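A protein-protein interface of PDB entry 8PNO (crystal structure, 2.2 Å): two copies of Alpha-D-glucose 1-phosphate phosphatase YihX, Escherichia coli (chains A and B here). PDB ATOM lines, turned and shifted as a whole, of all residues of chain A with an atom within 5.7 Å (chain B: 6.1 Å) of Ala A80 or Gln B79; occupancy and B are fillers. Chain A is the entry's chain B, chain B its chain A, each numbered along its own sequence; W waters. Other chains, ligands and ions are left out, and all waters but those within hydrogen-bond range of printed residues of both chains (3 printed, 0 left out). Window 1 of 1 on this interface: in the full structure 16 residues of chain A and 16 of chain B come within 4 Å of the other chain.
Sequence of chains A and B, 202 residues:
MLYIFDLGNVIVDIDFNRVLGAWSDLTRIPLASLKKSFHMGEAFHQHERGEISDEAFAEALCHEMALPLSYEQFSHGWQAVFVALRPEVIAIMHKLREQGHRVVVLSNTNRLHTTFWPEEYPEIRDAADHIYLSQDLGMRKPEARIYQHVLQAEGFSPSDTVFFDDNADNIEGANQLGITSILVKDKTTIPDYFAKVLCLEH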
ATOM      1  N   ASP A  15      27.622  29.977 -15.553  1.00  0.00           N
ATOM      2  CA  ASP A  15      27.141  30.223 -14.206  1.00  0.00           C
ATOM      3  C   ASP A  15      27.918  29.366 -13.201  1.00  0.00           C
ATOM      4  O   ASP A  15      27.712  28.160 -13.134  1.00  0.00           O
ATOM      5  CB  ASP A  15      25.628  30.016 -14.144  1.00  0.00           C
ATOM      6  CG  ASP A  15      24.979  30.553 -12.878  1.00  0.00           C
ATOM      7  OD1 ASP A  15      25.692  30.820 -11.887  1.00  0.00           O
ATOM      8  OD2 ASP A  15      23.753  30.720 -12.896  1.00  0.00           O
ATOM      9  N   ARG A  18      26.487  26.861 -10.149  1.00  0.00           N
ATOM     10  CA  ARG A  18      26.383  25.421 -10.320  1.00  0.00           C
ATOM     11  C   ARG A  18      27.564  24.705  -9.661  1.00  0.00           C
ATOM     12  O   ARG A  18      27.385  23.617  -9.128  1.00  0.00           O
ATOM     13  CB  ARG A  18      26.307  25.110 -11.816  1.00  0.00           C
ATOM     14  CG  ARG A  18      25.940  23.668 -12.147  1.00  0.00           C
ATOM     15  CD  ARG A  18      24.493  23.279 -11.914  1.00  0.00           C
ATOM     16  NE  ARG A  18      23.481  24.022 -12.686  1.00  0.00           N
ATOM     17  CZ  ARG A  18      23.043  23.695 -13.900  1.00  0.00           C
ATOM     18  NH1 ARG A  18      23.693  22.804 -14.629  1.00  0.00           N
ATOM     19  NH2 ARG A  18      21.979  24.306 -14.402  1.00  0.00           N
ATOM     20  N   VAL A  19      28.758  25.323  -9.712  1.00  0.00           N
ATOM     21  CA  VAL A  19      29.952  24.829  -9.031  1.00  0.00           C
ATOM     22  C   VAL A  19      29.722  24.829  -7.517  1.00  0.00           C
ATOM     23  O   VAL A  19      30.119  23.877  -6.835  1.00  0.00           O
ATOM     24  CB  VAL A  19      31.227  25.629  -9.409  1.00  0.00           C
ATOM     25  CG1 VAL A  19      32.466  25.175  -8.616  1.00  0.00           C
ATOM     26  CG2 VAL A  19      31.524  25.550 -10.907  1.00  0.00           C
ATOM     27  N   ALA A  22      27.554  22.062  -6.624  1.00  0.00           N
ATOM     28  CA  ALA A  22      28.291  20.805  -6.665  1.00  0.00           C
ATOM     29  C   ALA A  22      29.157  20.623  -5.421  1.00  0.00           C
ATOM     30  O   ALA A  22      29.226  19.525  -4.860  1.00  0.00           O
ATOM     31  CB  ALA A  22      29.155  20.763  -7.906  1.00  0.00           C
ATOM     32  N   SER A  75      38.262  19.934  -8.591  1.00  0.00           N
ATOM     33  CA  SER A  75      38.205  19.976 -10.046  1.00  0.00           C
ATOM     34  C   SER A  75      36.859  19.426 -10.520  1.00  0.00           C
ATOM     35  O   SER A  75      36.212  19.952 -11.429  1.00  0.00           O
ATOM     36  CB  SER A  75      39.387  19.179 -10.632  1.00  0.00           C
ATOM     37  OG  SER A  75      39.415  19.185 -12.060  1.00  0.00           O
ATOM     38  N   HIS A  76      36.472  18.330  -9.875  1.00  0.00           N
ATOM     39  CA  HIS A  76      35.237  17.614 -10.149  1.00  0.00           C
ATOM     40  C   HIS A  76      34.046  18.582 -10.067  1.00  0.00           C
ATOM     41  O   HIS A  76      33.180  18.574 -10.937  1.00  0.00           O
ATOM     42  CB  HIS A  76      35.213  16.375  -9.231  1.00  0.00           C
ATOM     43  CG  HIS A  76      34.151  15.390  -9.500  1.00  0.00           C
ATOM     44  ND1 HIS A  76      32.816  15.710  -9.424  1.00  0.00           N
ATOM     45  CD2 HIS A  76      34.220  14.078  -9.813  1.00  0.00           C
ATOM     46  CE1 HIS A  76      32.092  14.629  -9.721  1.00  0.00           C
ATOM     47  NE2 HIS A  76      32.927  13.619  -9.959  1.00  0.00           N
ATOM     48  N   GLY A  77      33.986  19.403  -9.007  1.00  0.00           N
ATOM     49  CA  GLY A  77      32.926  20.388  -8.880  1.00  0.00           C
ATOM     50  C   GLY A  77      33.069  21.538  -9.878  1.00  0.00           C
ATOM     51  O   GLY A  77      32.085  22.012 -10.429  1.00  0.00           O
ATOM     52  N   TRP A  78      34.312  21.999 -10.059  1.00  0.00           N
ATOM     53  CA  TRP A  78      34.673  23.012 -11.042  1.00  0.00           C
ATOM     54  C   TRP A  78      34.097  22.674 -12.418  1.00  0.00           C
ATOM     55  O   TRP A  78      33.516  23.537 -13.110  1.00  0.00           O
ATOM     56  CB  TRP A  78      36.211  23.145 -11.075  1.00  0.00           C
ATOM     57  CG  TRP A  78      36.713  24.469 -11.557  1.00  0.00           C
ATOM     58  CD1 TRP A  78      37.490  24.697 -12.653  1.00  0.00           C
ATOM     59  CD2 TRP A  78      36.484  25.751 -10.946  1.00  0.00           C
ATOM     60  NE1 TRP A  78      37.747  26.034 -12.780  1.00  0.00           N
ATOM     61  CE2 TRP A  78      37.147  26.707 -11.744  1.00  0.00           C
ATOM     62  CE3 TRP A  78      35.795  26.181  -9.804  1.00  0.00           C
ATOM     63  CZ2 TRP A  78      37.139  28.069 -11.433  1.00  0.00           C
ATOM     64  CZ3 TRP A  78      35.812  27.515  -9.485  1.00  0.00           C
ATOM     65  CH2 TRP A  78      36.463  28.449 -10.295  1.00  0.00           C
ATOM     66  N   GLN A  79      34.275  21.400 -12.789  1.00  0.00           N
ATOM     67  CA  GLN A  79      33.740  20.854 -14.031  1.00  0.00           C
ATOM     68  C   GLN A  79      32.224  21.060 -14.210  1.00  0.00           C
ATOM     69  O   GLN A  79      31.725  20.966 -15.344  1.00  0.00           O
ATOM     70  CB  GLN A  79      34.079  19.365 -14.104  1.00  0.00           C
ATOM     71  CG  GLN A  79      33.685  18.713 -15.426  1.00  0.00           C
ATOM     72  CD  GLN A  79      34.449  19.299 -16.583  1.00  0.00           C
ATOM     73  OE1 GLN A  79      35.604  18.929 -16.815  1.00  0.00           O
ATOM     74  NE2 GLN A  79      33.796  20.217 -17.292  1.00  0.00           N
ATOM     75  N   ALA A  80      31.479  21.290 -13.115  1.00  0.00           N
ATOM     76  CA  ALA A  80      30.027  21.337 -13.195  1.00  0.00           C
ATOM     77  C   ALA A  80      29.540  22.699 -13.684  1.00  0.00           C
ATOM     78  O   ALA A  80      28.339  22.883 -13.853  1.00  0.00           O
ATOM     79  CB  ALA A  80      29.402  20.989 -11.865  1.00  0.00           C
ATOM     80  N   VAL A  81      30.450  23.637 -13.964  1.00  0.00           N
ATOM     81  CA  VAL A  81      30.031  25.009 -14.249  1.00  0.00           C
ATOM     82  C   VAL A  81      29.042  24.978 -15.407  1.00  0.00           C
ATOM     83  O   VAL A  81      29.287  24.302 -16.412  1.00  0.00           O
ATOM     84  CB  VAL A  81      31.201  25.988 -14.528  1.00  0.00           C
ATOM     85  CG1 VAL A  81      32.138  25.552 -15.646  1.00  0.00           C
ATOM     86  CG2 VAL A  81      30.692  27.382 -14.836  1.00  0.00           C
ATOM     87  N   PHE A  82      27.933  25.702 -15.244  1.00  0.00           N
ATOM     88  CA  PHE A  82      26.912  25.783 -16.280  1.00  0.00           C
ATOM     89  C   PHE A  82      27.448  26.546 -17.492  1.00  0.00           C
ATOM     90  O   PHE A  82      27.867  27.697 -17.362  1.00  0.00           O
ATOM     91  CB  PHE A  82      25.651  26.464 -15.750  1.00  0.00           C
ATOM     92  CG  PHE A  82      24.611  26.692 -16.818  1.00  0.00           C
ATOM     93  CD1 PHE A  82      23.887  25.626 -17.335  1.00  0.00           C
ATOM     94  CD2 PHE A  82      24.397  27.958 -17.355  1.00  0.00           C
ATOM     95  CE1 PHE A  82      22.957  25.823 -18.343  1.00  0.00           C
ATOM     96  CE2 PHE A  82      23.460  28.153 -18.358  1.00  0.00           C
ATOM     97  CZ  PHE A  82      22.747  27.087 -18.857  1.00  0.00           C
ATOM     98  N   VAL B  19      29.258  15.309 -21.823  1.00  0.00           N
ATOM     99  CA  VAL B  19      30.048  14.257 -21.173  1.00  0.00           C
ATOM    100  C   VAL B  19      31.035  13.618 -22.159  1.00  0.00           C
ATOM    101  O   VAL B  19      32.187  13.388 -21.794  1.00  0.00           O
ATOM    102  CB  VAL B  19      29.166  13.161 -20.530  1.00  0.00           C
ATOM    103  CG1 VAL B  19      29.993  11.998 -19.979  1.00  0.00           C
ATOM    104  CG2 VAL B  19      28.254  13.718 -19.445  1.00  0.00           C
ATOM    105  N   PHE B  74      36.003   9.081 -14.910  1.00  0.00           N
ATOM    106  CA  PHE B  74      34.661   8.804 -15.387  1.00  0.00           C
ATOM    107  C   PHE B  74      33.673   9.816 -14.799  1.00  0.00           C
ATOM    108  O   PHE B  74      32.941  10.479 -15.537  1.00  0.00           O
ATOM    109  CB  PHE B  74      34.220   7.390 -14.990  1.00  0.00           C
ATOM    110  CG  PHE B  74      32.903   6.983 -15.600  1.00  0.00           C
ATOM    111  CD1 PHE B  74      32.833   6.568 -16.928  1.00  0.00           C
ATOM    112  CD2 PHE B  74      31.738   7.003 -14.848  1.00  0.00           C
ATOM    113  CE1 PHE B  74      31.621   6.192 -17.488  1.00  0.00           C
ATOM    114  CE2 PHE B  74      30.521   6.653 -15.415  1.00  0.00           C
ATOM    115  CZ  PHE B  74      30.460   6.257 -16.735  1.00  0.00           C
ATOM    116  N   SER B  75      33.662   9.891 -13.458  1.00  0.00           N
ATOM    117  CA  SER B  75      32.696  10.678 -12.711  1.00  0.00           C
ATOM    118  C   SER B  75      32.922  12.146 -13.059  1.00  0.00           C
ATOM    119  O   SER B  75      31.986  12.950 -13.222  1.00  0.00           O
ATOM    120  CB  SER B  75      32.818  10.409 -11.193  1.00  0.00           C
ATOM    121  OG  SER B  75      31.864  11.150 -10.409  1.00  0.00           O
ATOM    122  N   HIS B  76      34.200  12.472 -13.155  1.00  0.00           N
ATOM    123  CA  HIS B  76      34.602  13.840 -13.423  1.00  0.00           C
ATOM    124  C   HIS B  76      33.934  14.347 -14.707  1.00  0.00           C
ATOM    125  O   HIS B  76      33.412  15.464 -14.733  1.00  0.00           O
ATOM    126  CB  HIS B  76      36.137  13.893 -13.437  1.00  0.00           C
ATOM    127  CG  HIS B  76      36.690  15.253 -13.348  1.00  0.00           C
ATOM    128  ND1 HIS B  76      36.523  16.202 -14.338  1.00  0.00           N
ATOM    129  CD2 HIS B  76      37.429  15.805 -12.379  1.00  0.00           C
ATOM    130  CE1 HIS B  76      37.157  17.309 -13.965  1.00  0.00           C
ATOM    131  NE2 HIS B  76      37.739  17.075 -12.785  1.00  0.00           N
ATOM    132  N   GLY B  77      34.002  13.523 -15.777  1.00  0.00           N
ATOM    133  CA  GLY B  77      33.384  13.848 -17.053  1.00  0.00           C
ATOM    134  C   GLY B  77      31.864  13.672 -17.087  1.00  0.00           C
ATOM    135  O   GLY B  77      31.189  14.402 -17.807  1.00  0.00           O
ATOM    136  N   TRP B  78      31.369  12.644 -16.378  1.00  0.00           N
ATOM    137  CA  TRP B  78      29.948  12.437 -16.109  1.00  0.00           C
ATOM    138  C   TRP B  78      29.318  13.722 -15.572  1.00  0.00           C
ATOM    139  O   TRP B  78      28.254  14.151 -16.043  1.00  0.00           O
ATOM    140  CB  TRP B  78      29.739  11.256 -15.131  1.00  0.00           C
ATOM    141  CG  TRP B  78      28.402  10.572 -15.227  1.00  0.00           C
ATOM    142  CD1 TRP B  78      27.468  10.453 -14.228  1.00  0.00           C
ATOM    143  CD2 TRP B  78      27.865   9.855 -16.357  1.00  0.00           C
ATOM    144  NE1 TRP B  78      26.378   9.748 -14.661  1.00  0.00           N
ATOM    145  CE2 TRP B  78      26.598   9.355 -15.963  1.00  0.00           C
ATOM    146  CE3 TRP B  78      28.326   9.586 -17.659  1.00  0.00           C
ATOM    147  CZ2 TRP B  78      25.787   8.623 -16.839  1.00  0.00           C
ATOM    148  CZ3 TRP B  78      27.527   8.858 -18.511  1.00  0.00           C
ATOM    149  CH2 TRP B  78      26.271   8.396 -18.111  1.00  0.00           C
ATOM    150  N   GLN B  79      29.986  14.301 -14.570  1.00  0.00           N
ATOM    151  CA  GLN B  79      29.567  15.559 -13.960  1.00  0.00           C
ATOM    152  C   GLN B  79      29.407  16.738 -14.944  1.00  0.00           C
ATOM    153  O   GLN B  79      28.804  17.754 -14.566  1.00  0.00           O
ATOM    154  CB  GLN B  79      30.587  15.918 -12.885  1.00  0.00           C
ATOM    155  CG  GLN B  79      30.287  17.202 -12.141  1.00  0.00           C
ATOM    156  CD  GLN B  79      29.066  17.034 -11.276  1.00  0.00           C
ATOM    157  OE1 GLN B  79      29.137  16.417 -10.210  1.00  0.00           O
ATOM    158  NE2 GLN B  79      27.960  17.591 -11.744  1.00  0.00           N
ATOM    159  N   ALA B  80      29.960  16.648 -16.173  1.00  0.00           N
ATOM    160  CA  ALA B  80      29.927  17.769 -17.109  1.00  0.00           C
ATOM    161  C   ALA B  80      28.604  17.830 -17.864  1.00  0.00           C
ATOM    162  O   ALA B  80      28.390  18.772 -18.627  1.00  0.00           O
ATOM    163  CB  ALA B  80      31.056  17.714 -18.098  1.00  0.00           C
ATOM    164  N   VAL B  81      27.722  16.848 -17.659  1.00  0.00           N
ATOM    165  CA  VAL B  81      26.510  16.780 -18.459  1.00  0.00           C
ATOM    166  C   VAL B  81      25.834  18.147 -18.470  1.00  0.00           C
ATOM    167  O   VAL B  81      25.621  18.754 -17.413  1.00  0.00           O
ATOM    168  CB  VAL B  81      25.537  15.679 -17.987  1.00  0.00           C
ATOM    169  CG1 VAL B  81      25.089  15.842 -16.537  1.00  0.00           C
ATOM    170  CG2 VAL B  81      24.324  15.618 -18.893  1.00  0.00           C
ATOM    171  N   THR B 114      29.165  10.277  -6.515  1.00  0.00           N
ATOM    172  CA  THR B 114      30.129  11.382  -6.495  1.00  0.00           C
ATOM    173  C   THR B 114      29.673  12.607  -7.288  1.00  0.00           C
ATOM    174  O   THR B 114      30.419  13.568  -7.392  1.00  0.00           O
ATOM    175  CB  THR B 114      31.487  10.949  -7.052  1.00  0.00           C
ATOM    176  OG1 THR B 114      31.189  10.094  -8.168  1.00  0.00           O
ATOM    177  CG2 THR B 114      32.343  10.243  -6.017  1.00  0.00           C
ATOM    178  N   THR B 115      28.472  12.590  -7.856  1.00  0.00           N
ATOM    179  CA  THR B 115      28.064  13.647  -8.762  1.00  0.00           C
ATOM    180  C   THR B 115      26.897  14.433  -8.170  1.00  0.00           C
ATOM    181  O   THR B 115      26.123  13.931  -7.357  1.00  0.00           O
ATOM    182  CB  THR B 115      27.672  13.080 -10.136  1.00  0.00           C
ATOM    183  OG1 THR B 115      26.611  12.143  -9.954  1.00  0.00           O
ATOM    184  CG2 THR B 115      28.818  12.399 -10.863  1.00  0.00           C
ATOM    185  N   PHE B 116      26.809  15.683  -8.607  1.00  0.00           N
ATOM    186  CA  PHE B 116      25.724  16.598  -8.298  1.00  0.00           C
ATOM    187  C   PHE B 116      24.779  16.570  -9.500  1.00  0.00           C
ATOM    188  O   PHE B 116      25.222  16.898 -10.612  1.00  0.00           O
ATOM    189  CB  PHE B 116      26.287  17.996  -8.018  1.00  0.00           C
ATOM    190  CG  PHE B 116      25.243  19.054  -7.761  1.00  0.00           C
ATOM    191  CD1 PHE B 116      24.223  18.839  -6.845  1.00  0.00           C
ATOM    192  CD2 PHE B 116      25.292  20.277  -8.416  1.00  0.00           C
ATOM    193  CE1 PHE B 116      23.287  19.829  -6.596  1.00  0.00           C
ATOM    194  CE2 PHE B 116      24.352  21.267  -8.163  1.00  0.00           C
ATOM    195  CZ  PHE B 116      23.359  21.039  -7.247  1.00  0.00           C
ATOM    196  N   TRP B 117      23.521  16.123  -9.273  1.00  0.00           N
ATOM    197  CA  TRP B 117      22.636  15.746 -10.366  1.00  0.00           C
ATOM    198  C   TRP B 117      21.345  16.556 -10.243  1.00  0.00           C
ATOM    199  O   TRP B 117      21.064  17.015  -9.141  1.00  0.00           O
ATOM    200  CB  TRP B 117      22.408  14.226 -10.318  1.00  0.00           C
ATOM    201  CG  TRP B 117      22.497  13.465 -11.610  1.00  0.00           C
ATOM    202  CD1 TRP B 117      21.549  12.620 -12.120  1.00  0.00           C
ATOM    203  CD2 TRP B 117      23.620  13.380 -12.510  1.00  0.00           C
ATOM    204  NE1 TRP B 117      21.978  12.059 -13.287  1.00  0.00           N
ATOM    205  CE2 TRP B 117      23.248  12.498 -13.551  1.00  0.00           C
ATOM    206  CE3 TRP B 117      24.906  13.941 -12.528  1.00  0.00           C
ATOM    207  CZ2 TRP B 117      24.099  12.200 -14.617  1.00  0.00           C
ATOM    208  CZ3 TRP B 117      25.743  13.661 -13.589  1.00  0.00           C
ATOM    209  CH2 TRP B 117      25.330  12.816 -14.625  1.00  0.00           C
HETATM  210  O   HOH W   1      25.479  21.799 -16.818  1.00  0.00           O
HETATM  211  O   HOH W   2      36.216  16.288 -17.468  1.00  0.00           O
HETATM  212  O   HOH W   3      30.734  17.368  -7.977  1.00  0.00           O
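The side-chain hydroxyl (OG) of Ser B75 sits at hydrogen-bond distance from a ring nitrogen (NE2) of His A76 (2.7 Å).
NE2 of His B76 lies within hydrogen-bond range of OG of Ser A75, 2.8 Å away.
The backbone NH of His A76 lies within hydrogen-bond range of a ring nitrogen (NE2) of His B76 (3.4 Å).
OG of Ser B75 sits at hydrogen-bond distance from OG1 of Thr B114, 2.6 Å away.
OE1 of Gln B79 is in hydrogen-bond range of N of Phe B116 (2.9 Å).
Arg A18 touches Phe B116 (O to CE2, 3.96 Å).
N of Ala A22 touches CD2 of Phe B116 (3.4 Å).
Gln B79 touches His A76.
His A76 touches Thr B114.
O of His B76 touches CG of Gln A79 (3.3 Å).
Gln A79 touches Ala B80 (NE2 to CB, 3.8 Å).
CB of Ala A80 touches NE2 of Gln B79, 3.7 Å away.
Asp A15 touches none of the printed residues of chain B.
Val A19 touches none of the printed residues of chain B.
Of the printed residues of chain B, Ser A75 touches His B76.
Of the printed residues of chain B, His A76 touches Ser B75 (2.7 Å), His B76 (3.4 Å), Gln B79 (3.4 Å) and Thr B114 (3.1 Å).
Ala A80 touches one residue of chain B.
Of the printed residues of chain A, His B76 touches Ser A75, His A76 and Gln A79.
Of the printed residues of chain A, Thr B114 touches His A76.
Printed residues of chain A within 4 Å of Phe B116: Arg A18 (3.96 Å) and Ala A22 (3.4 Å).
The nearest residue of chain B that does not touch Ala A80 is Ala B80 (5.3 Å).
The nearest printed residue of chain B that does not touch Ser A75 is Gln B79 (6.6 Å).
Of the 13 printed residues of chain B, 6 touch a printed residue of chain A.
Printed residues of chain B that touch a printed residue of chain A: Ser B75, His B76, Gln B79, Ala B80, Thr B114 and Phe B116.
Hydrophobic or aromatic side chains of chain B that line the printed part of chain A: His B76, Ala B80 and Phe B116.
Of the 12 printed residues of chain A, 6 touch a printed residue of chain B.
Along chain A the printed residues that touch a printed residue of chain B span positions 18 to 80.
Among the printed residues, no Asp or Glu carboxylate lies within 4 Å of a Lys or Arg side-chain nitrogen of the other chain.
Ser A75 touches His B76, and with the chains exchanged His A76 touches Ser B75.
His B76 touches its own counterpart, His A76.
His A76 touches Gln B79, and with the chains exchanged Gln A79 touches His B76.
Gln A79 touches Ala B80, and with the chains exchanged Ala A80 touches Gln B79.
Of the 10 pairs that touch across the chains among the printed residues, 7 have their exchanged pair printed and touching as well.
Water W2 lies within hydrogen-bond range of OE1 of Gln A79 (2.8 Å) and ND1 of His B76 (3.1 Å).
Water W3 bridges the side-chain amide oxygen of Gln B79 (2.9 Å) and a ring nitrogen (ND1) of His A76 (3.0 Å).
Water W1 lies within hydrogen-bond range of NH1 of Arg A18 (3.0 Å) and O of Val B81 (3.1 Å).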
